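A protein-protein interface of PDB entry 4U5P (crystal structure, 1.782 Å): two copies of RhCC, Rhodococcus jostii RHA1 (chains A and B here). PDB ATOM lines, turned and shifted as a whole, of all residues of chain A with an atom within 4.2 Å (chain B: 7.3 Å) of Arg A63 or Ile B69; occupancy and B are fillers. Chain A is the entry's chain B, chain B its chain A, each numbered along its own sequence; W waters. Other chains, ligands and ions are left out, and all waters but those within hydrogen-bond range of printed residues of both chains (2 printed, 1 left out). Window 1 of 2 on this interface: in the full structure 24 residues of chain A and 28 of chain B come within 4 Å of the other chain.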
ATOM      1  N   GLU A   4       7.605  -9.004 -40.000  1.00  0.00           N
ATOM      2  CA  GLU A   4       8.929  -8.437 -40.237  1.00  0.00           C
ATOM      3  C   GLU A   4       9.950  -9.531 -40.108  1.00  0.00           C
ATOM      4  O   GLU A   4       9.948 -10.271 -39.121  1.00  0.00           O
ATOM      5  CB  GLU A   4       9.273  -7.330 -39.244  1.00  0.00           C
ATOM      6  CG  GLU A   4       8.446  -6.077 -39.327  1.00  0.00           C
ATOM      7  CD  GLU A   4       8.844  -5.117 -38.220  1.00  0.00           C
ATOM      8  OE1 GLU A   4       8.495  -5.407 -37.061  1.00  0.00           O
ATOM      9  OE2 GLU A   4       9.535  -4.111 -38.498  1.00  0.00           O
ATOM     10  N   ILE A   5      10.818  -9.636 -41.103  1.00  0.00           N
ATOM     11  CA  ILE A   5      11.872 -10.623 -41.079  1.00  0.00           C
ATOM     12  C   ILE A   5      13.224  -9.938 -41.262  1.00  0.00           C
ATOM     13  O   ILE A   5      13.568  -9.467 -42.340  1.00  0.00           O
ATOM     14  CB  ILE A   5      11.646 -11.694 -42.145  1.00  0.00           C
ATOM     15  CG1 ILE A   5      10.271 -12.342 -41.931  1.00  0.00           C
ATOM     16  CG2 ILE A   5      12.765 -12.750 -42.069  1.00  0.00           C
ATOM     17  CD1 ILE A   5       9.934 -13.450 -42.905  1.00  0.00           C
ATOM     18  N   PHE A   6      13.979  -9.876 -40.173  1.00  0.00           N
ATOM     19  CA  PHE A   6      15.311  -9.296 -40.178  1.00  0.00           C
ATOM     20  C   PHE A   6      16.334 -10.380 -40.468  1.00  0.00           C
ATOM     21  O   PHE A   6      16.427 -11.334 -39.707  1.00  0.00           O
ATOM     22  CB  PHE A   6      15.603  -8.641 -38.825  1.00  0.00           C
ATOM     23  CG  PHE A   6      14.646  -7.535 -38.466  1.00  0.00           C
ATOM     24  CD1 PHE A   6      13.467  -7.803 -37.787  1.00  0.00           C
ATOM     25  CD2 PHE A   6      14.937  -6.226 -38.793  1.00  0.00           C
ATOM     26  CE1 PHE A   6      12.590  -6.777 -37.452  1.00  0.00           C
ATOM     27  CE2 PHE A   6      14.064  -5.199 -38.456  1.00  0.00           C
ATOM     28  CZ  PHE A   6      12.897  -5.481 -37.781  1.00  0.00           C
ATOM     29  N   MET A  51      23.220  -6.802 -35.479  1.00  0.00           N
ATOM     30  CA  MET A  51      22.338  -7.666 -34.676  1.00  0.00           C
ATOM     31  C   MET A  51      23.135  -8.325 -33.547  1.00  0.00           C
ATOM     32  O   MET A  51      24.018  -9.141 -33.810  1.00  0.00           O
ATOM     33  CB  MET A  51      21.686  -8.761 -35.538  1.00  0.00           C
ATOM     34  CG  MET A  51      20.919  -8.255 -36.770  1.00  0.00           C
ATOM     35  SD  MET A  51      20.113  -9.530 -37.789  1.00  0.00           S
ATOM     36  CE  MET A  51      18.781 -10.040 -36.712  1.00  0.00           C
ATOM     37  N   PHE A  61      21.892 -14.713 -37.893  1.00  0.00           N
ATOM     38  CA  PHE A  61      20.686 -14.700 -37.055  1.00  0.00           C
ATOM     39  C   PHE A  61      19.513 -14.062 -37.800  1.00  0.00           C
ATOM     40  O   PHE A  61      19.644 -12.981 -38.371  1.00  0.00           O
ATOM     41  CB  PHE A  61      20.973 -13.943 -35.761  1.00  0.00           C
ATOM     42  CG  PHE A  61      19.830 -13.927 -34.771  1.00  0.00           C
ATOM     43  CD1 PHE A  61      19.248 -15.101 -34.332  1.00  0.00           C
ATOM     44  CD2 PHE A  61      19.372 -12.730 -34.254  1.00  0.00           C
ATOM     45  CE1 PHE A  61      18.208 -15.082 -33.399  1.00  0.00           C
ATOM     46  CE2 PHE A  61      18.340 -12.703 -33.324  1.00  0.00           C
ATOM     47  CZ  PHE A  61      17.760 -13.887 -32.897  1.00  0.00           C
ATOM     48  N   VAL A  62      18.384 -14.766 -37.830  1.00  0.00           N
ATOM     49  CA  VAL A  62      17.147 -14.243 -38.411  1.00  0.00           C
ATOM     50  C   VAL A  62      16.139 -14.002 -37.293  1.00  0.00           C
ATOM     51  O   VAL A  62      15.792 -14.928 -36.568  1.00  0.00           O
ATOM     52  CB  VAL A  62      16.558 -15.206 -39.461  1.00  0.00           C
ATOM     53  CG1 VAL A  62      15.205 -14.704 -39.961  1.00  0.00           C
ATOM     54  CG2 VAL A  62      17.533 -15.377 -40.629  1.00  0.00           C
ATOM     55  N   ARG A  63      15.683 -12.760 -37.145  1.00  0.00           N
ATOM     56  CA  ARG A  63      14.730 -12.417 -36.100  1.00  0.00           C
ATOM     57  C   ARG A  63      13.397 -12.068 -36.753  1.00  0.00           C
ATOM     58  O   ARG A  63      13.345 -11.240 -37.668  1.00  0.00           O
ATOM     59  CB  ARG A  63      15.250 -11.260 -35.251  1.00  0.00           C
ATOM     60  CG  ARG A  63      14.427 -10.962 -33.999  1.00  0.00           C
ATOM     61  CD  ARG A  63      14.356 -12.180 -33.093  1.00  0.00           C
ATOM     62  NE  ARG A  63      13.829 -11.916 -31.757  1.00  0.00           N
ATOM     63  CZ  ARG A  63      12.540 -11.828 -31.449  1.00  0.00           C
ATOM     64  NH1 ARG A  63      11.618 -11.938 -32.400  1.00  0.00           N
ATOM     65  NH2 ARG A  63      12.179 -11.602 -30.185  1.00  0.00           N
ATOM     66  N   ILE A  64      12.333 -12.728 -36.302  1.00  0.00           N
ATOM     67  CA  ILE A  64      11.008 -12.533 -36.891  1.00  0.00           C
ATOM     68  C   ILE A  64      10.069 -11.967 -35.841  1.00  0.00           C
ATOM     69  O   ILE A  64       9.995 -12.464 -34.728  1.00  0.00           O
ATOM     70  CB  ILE A  64      10.437 -13.852 -37.454  1.00  0.00           C
ATOM     71  CG1 ILE A  64      11.407 -14.441 -38.485  1.00  0.00           C
ATOM     72  CG2 ILE A  64       9.059 -13.629 -38.113  1.00  0.00           C
ATOM     73  CD1 ILE A  64      11.124 -15.877 -38.834  1.00  0.00           C
ATOM     74  N   GLU A 102      14.549 -16.699 -34.002  1.00  0.00           N
ATOM     75  CA  GLU A 102      13.616 -16.473 -32.903  1.00  0.00           C
ATOM     76  C   GLU A 102      12.413 -15.750 -33.470  1.00  0.00           C
ATOM     77  O   GLU A 102      12.567 -14.983 -34.408  1.00  0.00           O
ATOM     78  CB  GLU A 102      14.265 -15.651 -31.794  1.00  0.00           C
ATOM     79  CG  GLU A 102      13.375 -15.363 -30.604  1.00  0.00           C
ATOM     80  CD  GLU A 102      14.134 -14.689 -29.470  1.00  0.00           C
ATOM     81  OE1 GLU A 102      15.066 -13.893 -29.737  1.00  0.00           O
ATOM     82  OE2 GLU A 102      13.801 -14.975 -28.305  1.00  0.00           O
ATOM     83  N   ILE A 103      11.234 -15.992 -32.907  1.00  0.00           N
ATOM     84  CA  ILE A 103       9.997 -15.428 -33.443  1.00  0.00           C
ATOM     85  C   ILE A 103       9.036 -15.102 -32.317  1.00  0.00           C
ATOM     86  O   ILE A 103       8.918 -15.869 -31.359  1.00  0.00           O
ATOM     87  CB  ILE A 103       9.322 -16.412 -34.431  1.00  0.00           C
ATOM     88  CG1 ILE A 103       8.042 -15.805 -35.016  1.00  0.00           C
ATOM     89  CG2 ILE A 103       9.007 -17.746 -33.737  1.00  0.00           C
ATOM     90  CD1 ILE A 103       7.486 -16.577 -36.215  1.00  0.00           C
ATOM     91  N   HIS A 104       8.349 -13.964 -32.407  1.00  0.00           N
ATOM     92  CA  HIS A 104       7.226 -13.732 -31.506  1.00  0.00           C
ATOM     93  C   HIS A 104       6.107 -12.950 -32.177  1.00  0.00           C
ATOM     94  O   HIS A 104       6.312 -12.325 -33.223  1.00  0.00           O
ATOM     95  CB  HIS A 104       7.675 -13.034 -30.215  1.00  0.00           C
ATOM     96  CG  HIS A 104       8.030 -11.586 -30.366  1.00  0.00           C
ATOM     97  ND1 HIS A 104       9.213 -11.167 -30.933  1.00  0.00           N
ATOM     98  CD2 HIS A 104       7.390 -10.465 -29.963  1.00  0.00           C
ATOM     99  CE1 HIS A 104       9.273  -9.848 -30.903  1.00  0.00           C
ATOM    100  NE2 HIS A 104       8.180  -9.397 -30.319  1.00  0.00           N
ATOM    101  N   PRO B   1      14.001 -10.202 -24.350  1.00  0.00           N
ATOM    102  CA  PRO B   1      13.824  -8.788 -24.701  1.00  0.00           C
ATOM    103  C   PRO B   1      14.255  -8.523 -26.129  1.00  0.00           C
ATOM    104  O   PRO B   1      15.251  -9.084 -26.588  1.00  0.00           O
ATOM    105  CB  PRO B   1      14.734  -8.059 -23.713  1.00  0.00           C
ATOM    106  CG  PRO B   1      14.821  -8.978 -22.547  1.00  0.00           C
ATOM    107  CD  PRO B   1      14.758 -10.364 -23.096  1.00  0.00           C
ATOM    108  N   TYR B   2      13.491  -7.677 -26.813  1.00  0.00           N
ATOM    109  CA  TYR B   2      13.703  -7.351 -28.206  1.00  0.00           C
ATOM    110  C   TYR B   2      13.870  -5.847 -28.317  1.00  0.00           C
ATOM    111  O   TYR B   2      12.886  -5.132 -28.222  1.00  0.00           O
ATOM    112  CB  TYR B   2      12.506  -7.860 -29.022  1.00  0.00           C
ATOM    113  CG  TYR B   2      12.403  -7.402 -30.459  1.00  0.00           C
ATOM    114  CD1 TYR B   2      13.126  -8.023 -31.462  1.00  0.00           C
ATOM    115  CD2 TYR B   2      11.540  -6.376 -30.820  1.00  0.00           C
ATOM    116  CE1 TYR B   2      13.016  -7.624 -32.781  1.00  0.00           C
ATOM    117  CE2 TYR B   2      11.422  -5.968 -32.128  1.00  0.00           C
ATOM    118  CZ  TYR B   2      12.161  -6.592 -33.106  1.00  0.00           C
ATOM    119  OH  TYR B   2      12.039  -6.182 -34.413  1.00  0.00           O
ATOM    120  N   TRP B   3      15.107  -5.382 -28.493  1.00  0.00           N
ATOM    121  CA  TRP B   3      15.434  -3.951 -28.541  1.00  0.00           C
ATOM    122  C   TRP B   3      15.728  -3.465 -29.961  1.00  0.00           C
ATOM    123  O   TRP B   3      16.548  -4.058 -30.657  1.00  0.00           O
ATOM    124  CB  TRP B   3      16.667  -3.656 -27.668  1.00  0.00           C
ATOM    125  CG  TRP B   3      16.450  -3.695 -26.179  1.00  0.00           C
ATOM    126  CD1 TRP B   3      15.966  -4.736 -25.447  1.00  0.00           C
ATOM    127  CD2 TRP B   3      16.744  -2.652 -25.240  1.00  0.00           C
ATOM    128  NE1 TRP B   3      15.935  -4.407 -24.116  1.00  0.00           N
ATOM    129  CE2 TRP B   3      16.411  -3.133 -23.962  1.00  0.00           C
ATOM    130  CE3 TRP B   3      17.258  -1.361 -25.359  1.00  0.00           C
ATOM    131  CZ2 TRP B   3      16.564  -2.366 -22.805  1.00  0.00           C
ATOM    132  CZ3 TRP B   3      17.415  -0.603 -24.211  1.00  0.00           C
ATOM    133  CH2 TRP B   3      17.066  -1.108 -22.951  1.00  0.00           C
ATOM    134  N   TYR B  38      18.563 -14.620 -24.665  1.00  0.00           N
ATOM    135  CA  TYR B  38      17.206 -14.072 -24.845  1.00  0.00           C
ATOM    136  C   TYR B  38      17.257 -12.619 -25.298  1.00  0.00           C
ATOM    137  O   TYR B  38      16.307 -12.118 -25.912  1.00  0.00           O
ATOM    138  CB  TYR B  38      16.377 -14.135 -23.564  1.00  0.00           C
ATOM    139  CG  TYR B  38      15.788 -15.474 -23.196  1.00  0.00           C
ATOM    140  CD1 TYR B  38      16.106 -16.635 -23.895  1.00  0.00           C
ATOM    141  CD2 TYR B  38      14.899 -15.570 -22.135  1.00  0.00           C
ATOM    142  CE1 TYR B  38      15.553 -17.857 -23.527  1.00  0.00           C
ATOM    143  CE2 TYR B  38      14.347 -16.774 -21.766  1.00  0.00           C
ATOM    144  CZ  TYR B  38      14.673 -17.912 -22.460  1.00  0.00           C
ATOM    145  OH  TYR B  38      14.105 -19.095 -22.053  1.00  0.00           O
ATOM    146  N   VAL B  40      18.093  -9.610 -27.422  1.00  0.00           N
ATOM    147  CA  VAL B  40      18.422  -9.233 -28.784  1.00  0.00           C
ATOM    148  C   VAL B  40      18.360  -7.715 -28.959  1.00  0.00           C
ATOM    149  O   VAL B  40      17.366  -7.090 -28.596  1.00  0.00           O
ATOM    150  CB  VAL B  40      17.462  -9.890 -29.787  1.00  0.00           C
ATOM    151  CG1 VAL B  40      17.782  -9.441 -31.213  1.00  0.00           C
ATOM    152  CG2 VAL B  40      17.540 -11.407 -29.668  1.00  0.00           C
ATOM    153  N   LEU B  42      18.950  -4.770 -31.927  1.00  0.00           N
ATOM    154  CA  LEU B  42      19.095  -4.431 -33.340  1.00  0.00           C
ATOM    155  C   LEU B  42      19.392  -2.945 -33.503  1.00  0.00           C
ATOM    156  O   LEU B  42      18.595  -2.094 -33.092  1.00  0.00           O
ATOM    157  CB  LEU B  42      17.818  -4.778 -34.110  1.00  0.00           C
ATOM    158  CG  LEU B  42      17.216  -6.180 -33.956  1.00  0.00           C
ATOM    159  CD1 LEU B  42      15.976  -6.316 -34.850  1.00  0.00           C
ATOM    160  CD2 LEU B  42      18.215  -7.267 -34.278  1.00  0.00           C
ATOM    161  N   ASP B  67      10.242  -4.694 -27.037  1.00  0.00           N
ATOM    162  CA  ASP B  67       9.218  -5.618 -26.566  1.00  0.00           C
ATOM    163  C   ASP B  67       9.754  -6.448 -25.403  1.00  0.00           C
ATOM    164  O   ASP B  67      10.880  -6.953 -25.459  1.00  0.00           O
ATOM    165  CB  ASP B  67       8.765  -6.585 -27.672  1.00  0.00           C
ATOM    166  CG  ASP B  67       7.913  -5.934 -28.737  1.00  0.00           C
ATOM    167  OD1 ASP B  67       7.261  -4.900 -28.462  1.00  0.00           O
ATOM    168  OD2 ASP B  67       7.868  -6.509 -29.846  1.00  0.00           O
ATOM    169  N   HIS B  68       8.941  -6.575 -24.363  1.00  0.00           N
ATOM    170  CA  HIS B  68       9.144  -7.558 -23.311  1.00  0.00           C
ATOM    171  C   HIS B  68       8.178  -8.712 -23.514  1.00  0.00           C
ATOM    172  O   HIS B  68       6.964  -8.511 -23.540  1.00  0.00           O
ATOM    173  CB  HIS B  68       8.938  -6.934 -21.940  1.00  0.00           C
ATOM    174  CG  HIS B  68      10.143  -6.232 -21.412  1.00  0.00           C
ATOM    175  ND1 HIS B  68      10.178  -5.669 -20.153  1.00  0.00           N
ATOM    176  CD2 HIS B  68      11.365  -6.011 -21.955  1.00  0.00           C
ATOM    177  CE1 HIS B  68      11.367  -5.136 -19.943  1.00  0.00           C
ATOM    178  NE2 HIS B  68      12.104  -5.324 -21.025  1.00  0.00           N
ATOM    179  N   ILE B  69       8.743  -9.909 -23.648  1.00  0.00           N
ATOM    180  CA  ILE B  69       8.010 -11.114 -24.004  1.00  0.00           C
ATOM    181  C   ILE B  69       8.003 -12.136 -22.875  1.00  0.00           C
ATOM    182  O   ILE B  69       6.970 -12.724 -22.558  1.00  0.00           O
ATOM    183  CB  ILE B  69       8.645 -11.800 -25.244  1.00  0.00           C
ATOM    184  CG1 ILE B  69       8.865 -10.803 -26.393  1.00  0.00           C
ATOM    185  CG2 ILE B  69       7.787 -12.973 -25.711  1.00  0.00           C
ATOM    186  CD1 ILE B  69       9.944 -11.249 -27.387  1.00  0.00           C
ATOM    187  N   ALA B  70       9.172 -12.339 -22.274  1.00  0.00           N
ATOM    188  CA  ALA B  70       9.376 -13.471 -21.375  1.00  0.00           C
ATOM    189  C   ALA B  70       8.541 -13.363 -20.095  1.00  0.00           C
ATOM    190  O   ALA B  70       7.974 -14.362 -19.640  1.00  0.00           O
ATOM    191  CB  ALA B  70      10.853 -13.588 -21.036  1.00  0.00           C
ATOM    192  N   ARG B  71       8.442 -12.164 -19.528  1.00  0.00           N
ATOM    193  CA  ARG B  71       7.622 -11.973 -18.334  1.00  0.00           C
ATOM    194  C   ARG B  71       6.943 -10.614 -18.331  1.00  0.00           C
ATOM    195  O   ARG B  71       7.246  -9.741 -19.147  1.00  0.00           O
ATOM    196  CB  ARG B  71       8.418 -12.122 -17.036  1.00  0.00           C
ATOM    197  CG  ARG B  71       9.695 -11.332 -16.954  1.00  0.00           C
ATOM    198  CD  ARG B  71      10.876 -12.211 -17.277  1.00  0.00           C
ATOM    199  NE  ARG B  71      11.159 -13.107 -16.149  1.00  0.00           N
ATOM    200  CZ  ARG B  71      11.585 -14.368 -16.248  1.00  0.00           C
ATOM    201  NH1 ARG B  71      11.813 -15.071 -15.145  1.00  0.00           N
ATOM    202  NH2 ARG B  71      11.778 -14.943 -17.433  1.00  0.00           N
ATOM    203  N   GLN B  72       6.044 -10.456 -17.366  1.00  0.00           N
ATOM    204  CA  GLN B  72       5.324  -9.214 -17.141  1.00  0.00           C
ATOM    205  C   GLN B  72       5.823  -8.536 -15.872  1.00  0.00           C
ATOM    206  O   GLN B  72       6.206  -9.209 -14.917  1.00  0.00           O
ATOM    207  CB  GLN B  72       3.822  -9.481 -17.021  1.00  0.00           C
ATOM    208  CG  GLN B  72       3.128  -9.827 -18.321  1.00  0.00           C
ATOM    209  CD  GLN B  72       1.623  -9.953 -18.150  1.00  0.00           C
ATOM    210  OE1 GLN B  72       1.145 -10.534 -17.176  1.00  0.00           O
ATOM    211  NE2 GLN B  72       0.867  -9.398 -19.095  1.00  0.00           N
ATOM    212  N   ASP B 106       6.762  -2.179 -25.065  1.00  0.00           N
ATOM    213  CA  ASP B 106       5.490  -2.894 -25.095  1.00  0.00           C
ATOM    214  C   ASP B 106       5.648  -4.278 -24.481  1.00  0.00           C
ATOM    215  O   ASP B 106       6.727  -4.869 -24.538  1.00  0.00           O
ATOM    216  CB  ASP B 106       4.967  -3.019 -26.515  1.00  0.00           C
ATOM    217  CG  ASP B 106       3.482  -3.369 -26.560  1.00  0.00           C
ATOM    218  OD1 ASP B 106       2.749  -3.041 -25.593  1.00  0.00           O
ATOM    219  OD2 ASP B 106       3.048  -3.964 -27.565  1.00  0.00           O
ATOM    220  N   GLU B 107       4.579  -4.785 -23.877  1.00  0.00           N
ATOM    221  CA  GLU B 107       4.576  -6.144 -23.348  1.00  0.00           C
ATOM    222  C   GLU B 107       3.713  -7.037 -24.228  1.00  0.00           C
ATOM    223  O   GLU B 107       2.536  -6.731 -24.462  1.00  0.00           O
ATOM    224  CB  GLU B 107       4.079  -6.158 -21.897  1.00  0.00           C
ATOM    225  CG  GLU B 107       4.999  -5.393 -20.929  1.00  0.00           C
ATOM    226  CD  GLU B 107       4.559  -5.490 -19.471  1.00  0.00           C
ATOM    227  OE1 GLU B 107       3.396  -5.162 -19.181  1.00  0.00           O
ATOM    228  OE2 GLU B 107       5.382  -5.888 -18.612  1.00  0.00           O
ATOM    229  N   THR B 108       4.296  -8.126 -24.723  1.00  0.00           N
ATOM    230  CA  THR B 108       3.620  -9.009 -25.684  1.00  0.00           C
ATOM    231  C   THR B 108       3.443 -10.407 -25.072  1.00  0.00           C
ATOM    232  O   THR B 108       4.114 -10.750 -24.094  1.00  0.00           O
ATOM    233  CB  THR B 108       4.412  -9.093 -27.022  1.00  0.00           C
ATOM    234  OG1 THR B 108       5.647  -9.774 -26.805  1.00  0.00           O
ATOM    235  CG2 THR B 108       4.709  -7.706 -27.567  1.00  0.00           C
ATOM    236  N   PRO B 109       2.505 -11.205 -25.609  1.00  0.00           N
ATOM    237  CA  PRO B 109       2.169 -12.499 -24.980  1.00  0.00           C
ATOM    238  C   PRO B 109       3.305 -13.539 -24.901  1.00  0.00           C
ATOM    239  O   PRO B 109       3.965 -13.851 -25.891  1.00  0.00           O
ATOM    240  CB  PRO B 109       1.016 -13.023 -25.856  1.00  0.00           C
ATOM    241  CG  PRO B 109       1.028 -12.194 -27.083  1.00  0.00           C
ATOM    242  CD  PRO B 109       1.590 -10.881 -26.715  1.00  0.00           C
ATOM    243  N   MET B 110       3.494 -14.098 -23.710  1.00  0.00           N
ATOM    244  CA  MET B 110       4.540 -15.098 -23.464  1.00  0.00           C
ATOM    245  C   MET B 110       4.395 -16.383 -24.262  1.00  0.00           C
ATOM    246  O   MET B 110       5.389 -17.027 -24.620  1.00  0.00           O
ATOM    247  CB  MET B 110       4.537 -15.464 -21.977  1.00  0.00           C
ATOM    248  CG  MET B 110       5.377 -16.675 -21.615  1.00  0.00           C
ATOM    249  SD  MET B 110       5.435 -16.919 -19.831  1.00  0.00           S
ATOM    250  CE  MET B 110       3.701 -17.347 -19.520  1.00  0.00           C
ATOM    251  N   ASP B 111       3.158 -16.753 -24.556  1.00  0.00           N
ATOM    252  CA  ASP B 111       2.906 -18.028 -25.197  1.00  0.00           C
ATOM    253  C   ASP B 111       2.981 -17.972 -26.734  1.00  0.00           C
ATOM    254  O   ASP B 111       2.848 -19.003 -27.376  1.00  0.00           O
ATOM    255  CB  ASP B 111       1.549 -18.577 -24.738  1.00  0.00           C
ATOM    256  CG  ASP B 111       0.366 -17.671 -25.094  1.00  0.00           C
ATOM    257  OD1 ASP B 111       0.548 -16.487 -25.448  1.00  0.00           O
ATOM    258  OD2 ASP B 111      -0.774 -18.154 -24.966  1.00  0.00           O
ATOM    259  N   LEU B 112       3.218 -16.794 -27.314  1.00  0.00           N
ATOM    260  CA  LEU B 112       3.376 -16.662 -28.775  1.00  0.00           C
ATOM    261  C   LEU B 112       4.835 -16.358 -29.110  1.00  0.00           C
ATOM    262  O   LEU B 112       5.149 -15.367 -29.753  1.00  0.00           O
ATOM    263  CB  LEU B 112       2.437 -15.570 -29.324  1.00  0.00           C
ATOM    264  CG  LEU B 112       0.944 -15.779 -29.037  1.00  0.00           C
ATOM    265  CD1 LEU B 112       0.088 -14.656 -29.631  1.00  0.00           C
ATOM    266  CD2 LEU B 112       0.468 -17.127 -29.552  1.00  0.00           C
ATOM    267  N   TRP B 113       5.729 -17.228 -28.648  1.00  0.00           N
ATOM    268  CA  TRP B 113       7.161 -16.963 -28.703  1.00  0.00           C
ATOM    269  C   TRP B 113       7.923 -18.290 -28.756  1.00  0.00           C
ATOM    270  O   TRP B 113       7.660 -19.206 -27.979  1.00  0.00           O
ATOM    271  CB  TRP B 113       7.563 -16.114 -27.486  1.00  0.00           C
ATOM    272  CG  TRP B 113       9.024 -16.008 -27.210  1.00  0.00           C
ATOM    273  CD1 TRP B 113      10.030 -15.787 -28.104  1.00  0.00           C
ATOM    274  CD2 TRP B 113       9.648 -16.138 -25.927  1.00  0.00           C
ATOM    275  NE1 TRP B 113      11.248 -15.771 -27.450  1.00  0.00           N
ATOM    276  CE2 TRP B 113      11.034 -15.980 -26.114  1.00  0.00           C
ATOM    277  CE3 TRP B 113       9.161 -16.370 -24.638  1.00  0.00           C
ATOM    278  CZ2 TRP B 113      11.944 -16.058 -25.054  1.00  0.00           C
ATOM    279  CZ3 TRP B 113      10.063 -16.438 -23.586  1.00  0.00           C
ATOM    280  CH2 TRP B 113      11.437 -16.282 -23.803  1.00  0.00           C
ATOM    281  N   ARG B 114       8.828 -18.406 -29.714  1.00  0.00           N
ATOM    282  CA  ARG B 114       9.681 -19.590 -29.845  1.00  0.00           C
ATOM    283  C   ARG B 114      11.101 -19.142 -30.124  1.00  0.00           C
ATOM    284  O   ARG B 114      11.317 -18.122 -30.767  1.00  0.00           O
ATOM    285  CB  ARG B 114       9.208 -20.519 -30.974  1.00  0.00           C
ATOM    286  CG  ARG B 114       7.773 -21.054 -30.844  1.00  0.00           C
ATOM    287  CD  ARG B 114       7.632 -22.129 -29.753  1.00  0.00           C
ATOM    288  NE  ARG B 114       6.270 -22.674 -29.651  1.00  0.00           N
ATOM    289  CZ  ARG B 114       5.306 -22.180 -28.869  1.00  0.00           C
ATOM    290  NH1 ARG B 114       5.523 -21.124 -28.088  1.00  0.00           N
ATOM    291  NH2 ARG B 114       4.111 -22.756 -28.851  1.00  0.00           N
HETATM  292  O   HOH W   1      13.928 -13.342 -26.331  1.00  0.00           O
HETATM  293  O   HOH W   2       9.875  -4.683 -35.095  1.00  0.00           O
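OD2 of Asp B67 is in hydrogen-bond range of NE2 of His A104 (2.9 Å).
The backbone NH (N) of Ile A103 sits at hydrogen-bond distance from the backbone carbonyl oxygen (O) of Arg B114 (3.0 Å).
The side-chain carboxylate (OE2) of Glu A102 lies within hydrogen-bond range of the indole nitrogen (NE1) of Trp B113.
The backbone NH of Phe A6 sits at hydrogen-bond distance from the backbone carbonyl oxygen of Arg A63.
The guanidinium group (NE) of Arg A63 is in salt-bridge range of the side-chain carboxylate (OE1) of Glu A102 (3.1 Å).
ND1 of His A104 is in hydrogen-bond range of NH1 of Arg A63, at 2.9 Å.
The backbone NH (N) of His A104 lies within hydrogen-bond range of the backbone carbonyl oxygen (O) of Ile A64, at 3.2 Å.
O of Tyr B2 is in hydrogen-bond range of N of Asp B67 (2.9 Å).
O of Glu A102 sits at hydrogen-bond distance from N of Ile A64.
Among the printed residues, merely in contact across the chains: Phe A6 with Tyr B2 (3.1 Å), His A104 with Leu B112 (3.2 Å), Ile A103 with Trp B113 (3.4 Å), Glu A102 with Arg B114 (3.4 Å), Glu A102 with Val B40 (3.5 Å), His A104 with Ile B69 (3.6 Å), Arg A63 with Ile B69 (3.6 Å), His A104 with Thr B108 (3.7 Å), Met A51 with Leu B42 (3.7 Å), Arg A63 with Tyr B2 (3.8 Å), Phe A61 with Val B40 (3.9 Å) and His A104 with Tyr B2 (3.997 Å).
Of the printed residues of chain B, Arg A63 touches Tyr B2 and Ile B69.
Printed residues of chain A within 4 Å of Ile B69: Arg A63 and His A104.
Of the printed residues of chain A, Leu B112 touches His A104.
Printed residues of chain A within 4 Å of Trp B113: Glu A102 (2.8 Å) and Ile A103 (3.4 Å).
The nearest printed residue of chain A that does not touch Ile B69 is Glu A102 (5.4 Å).
The nearest printed residue of chain A that does not touch Tyr B2 is Glu A4 (4.5 Å).
Of the 11 printed residues of chain A, 7 touch a printed residue of chain B.
Among the printed residues, 15 pairs touch across the chains.
No position is printed for both chains.
Water W2 lies within hydrogen-bond range of OE1 of Glu A4 (2.5 Å) and OH of Tyr B2 (2.7 Å).
Water W1 bridges OE2 of Glu A102 (2.6 Å) and O of Tyr B38 (2.7 Å).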
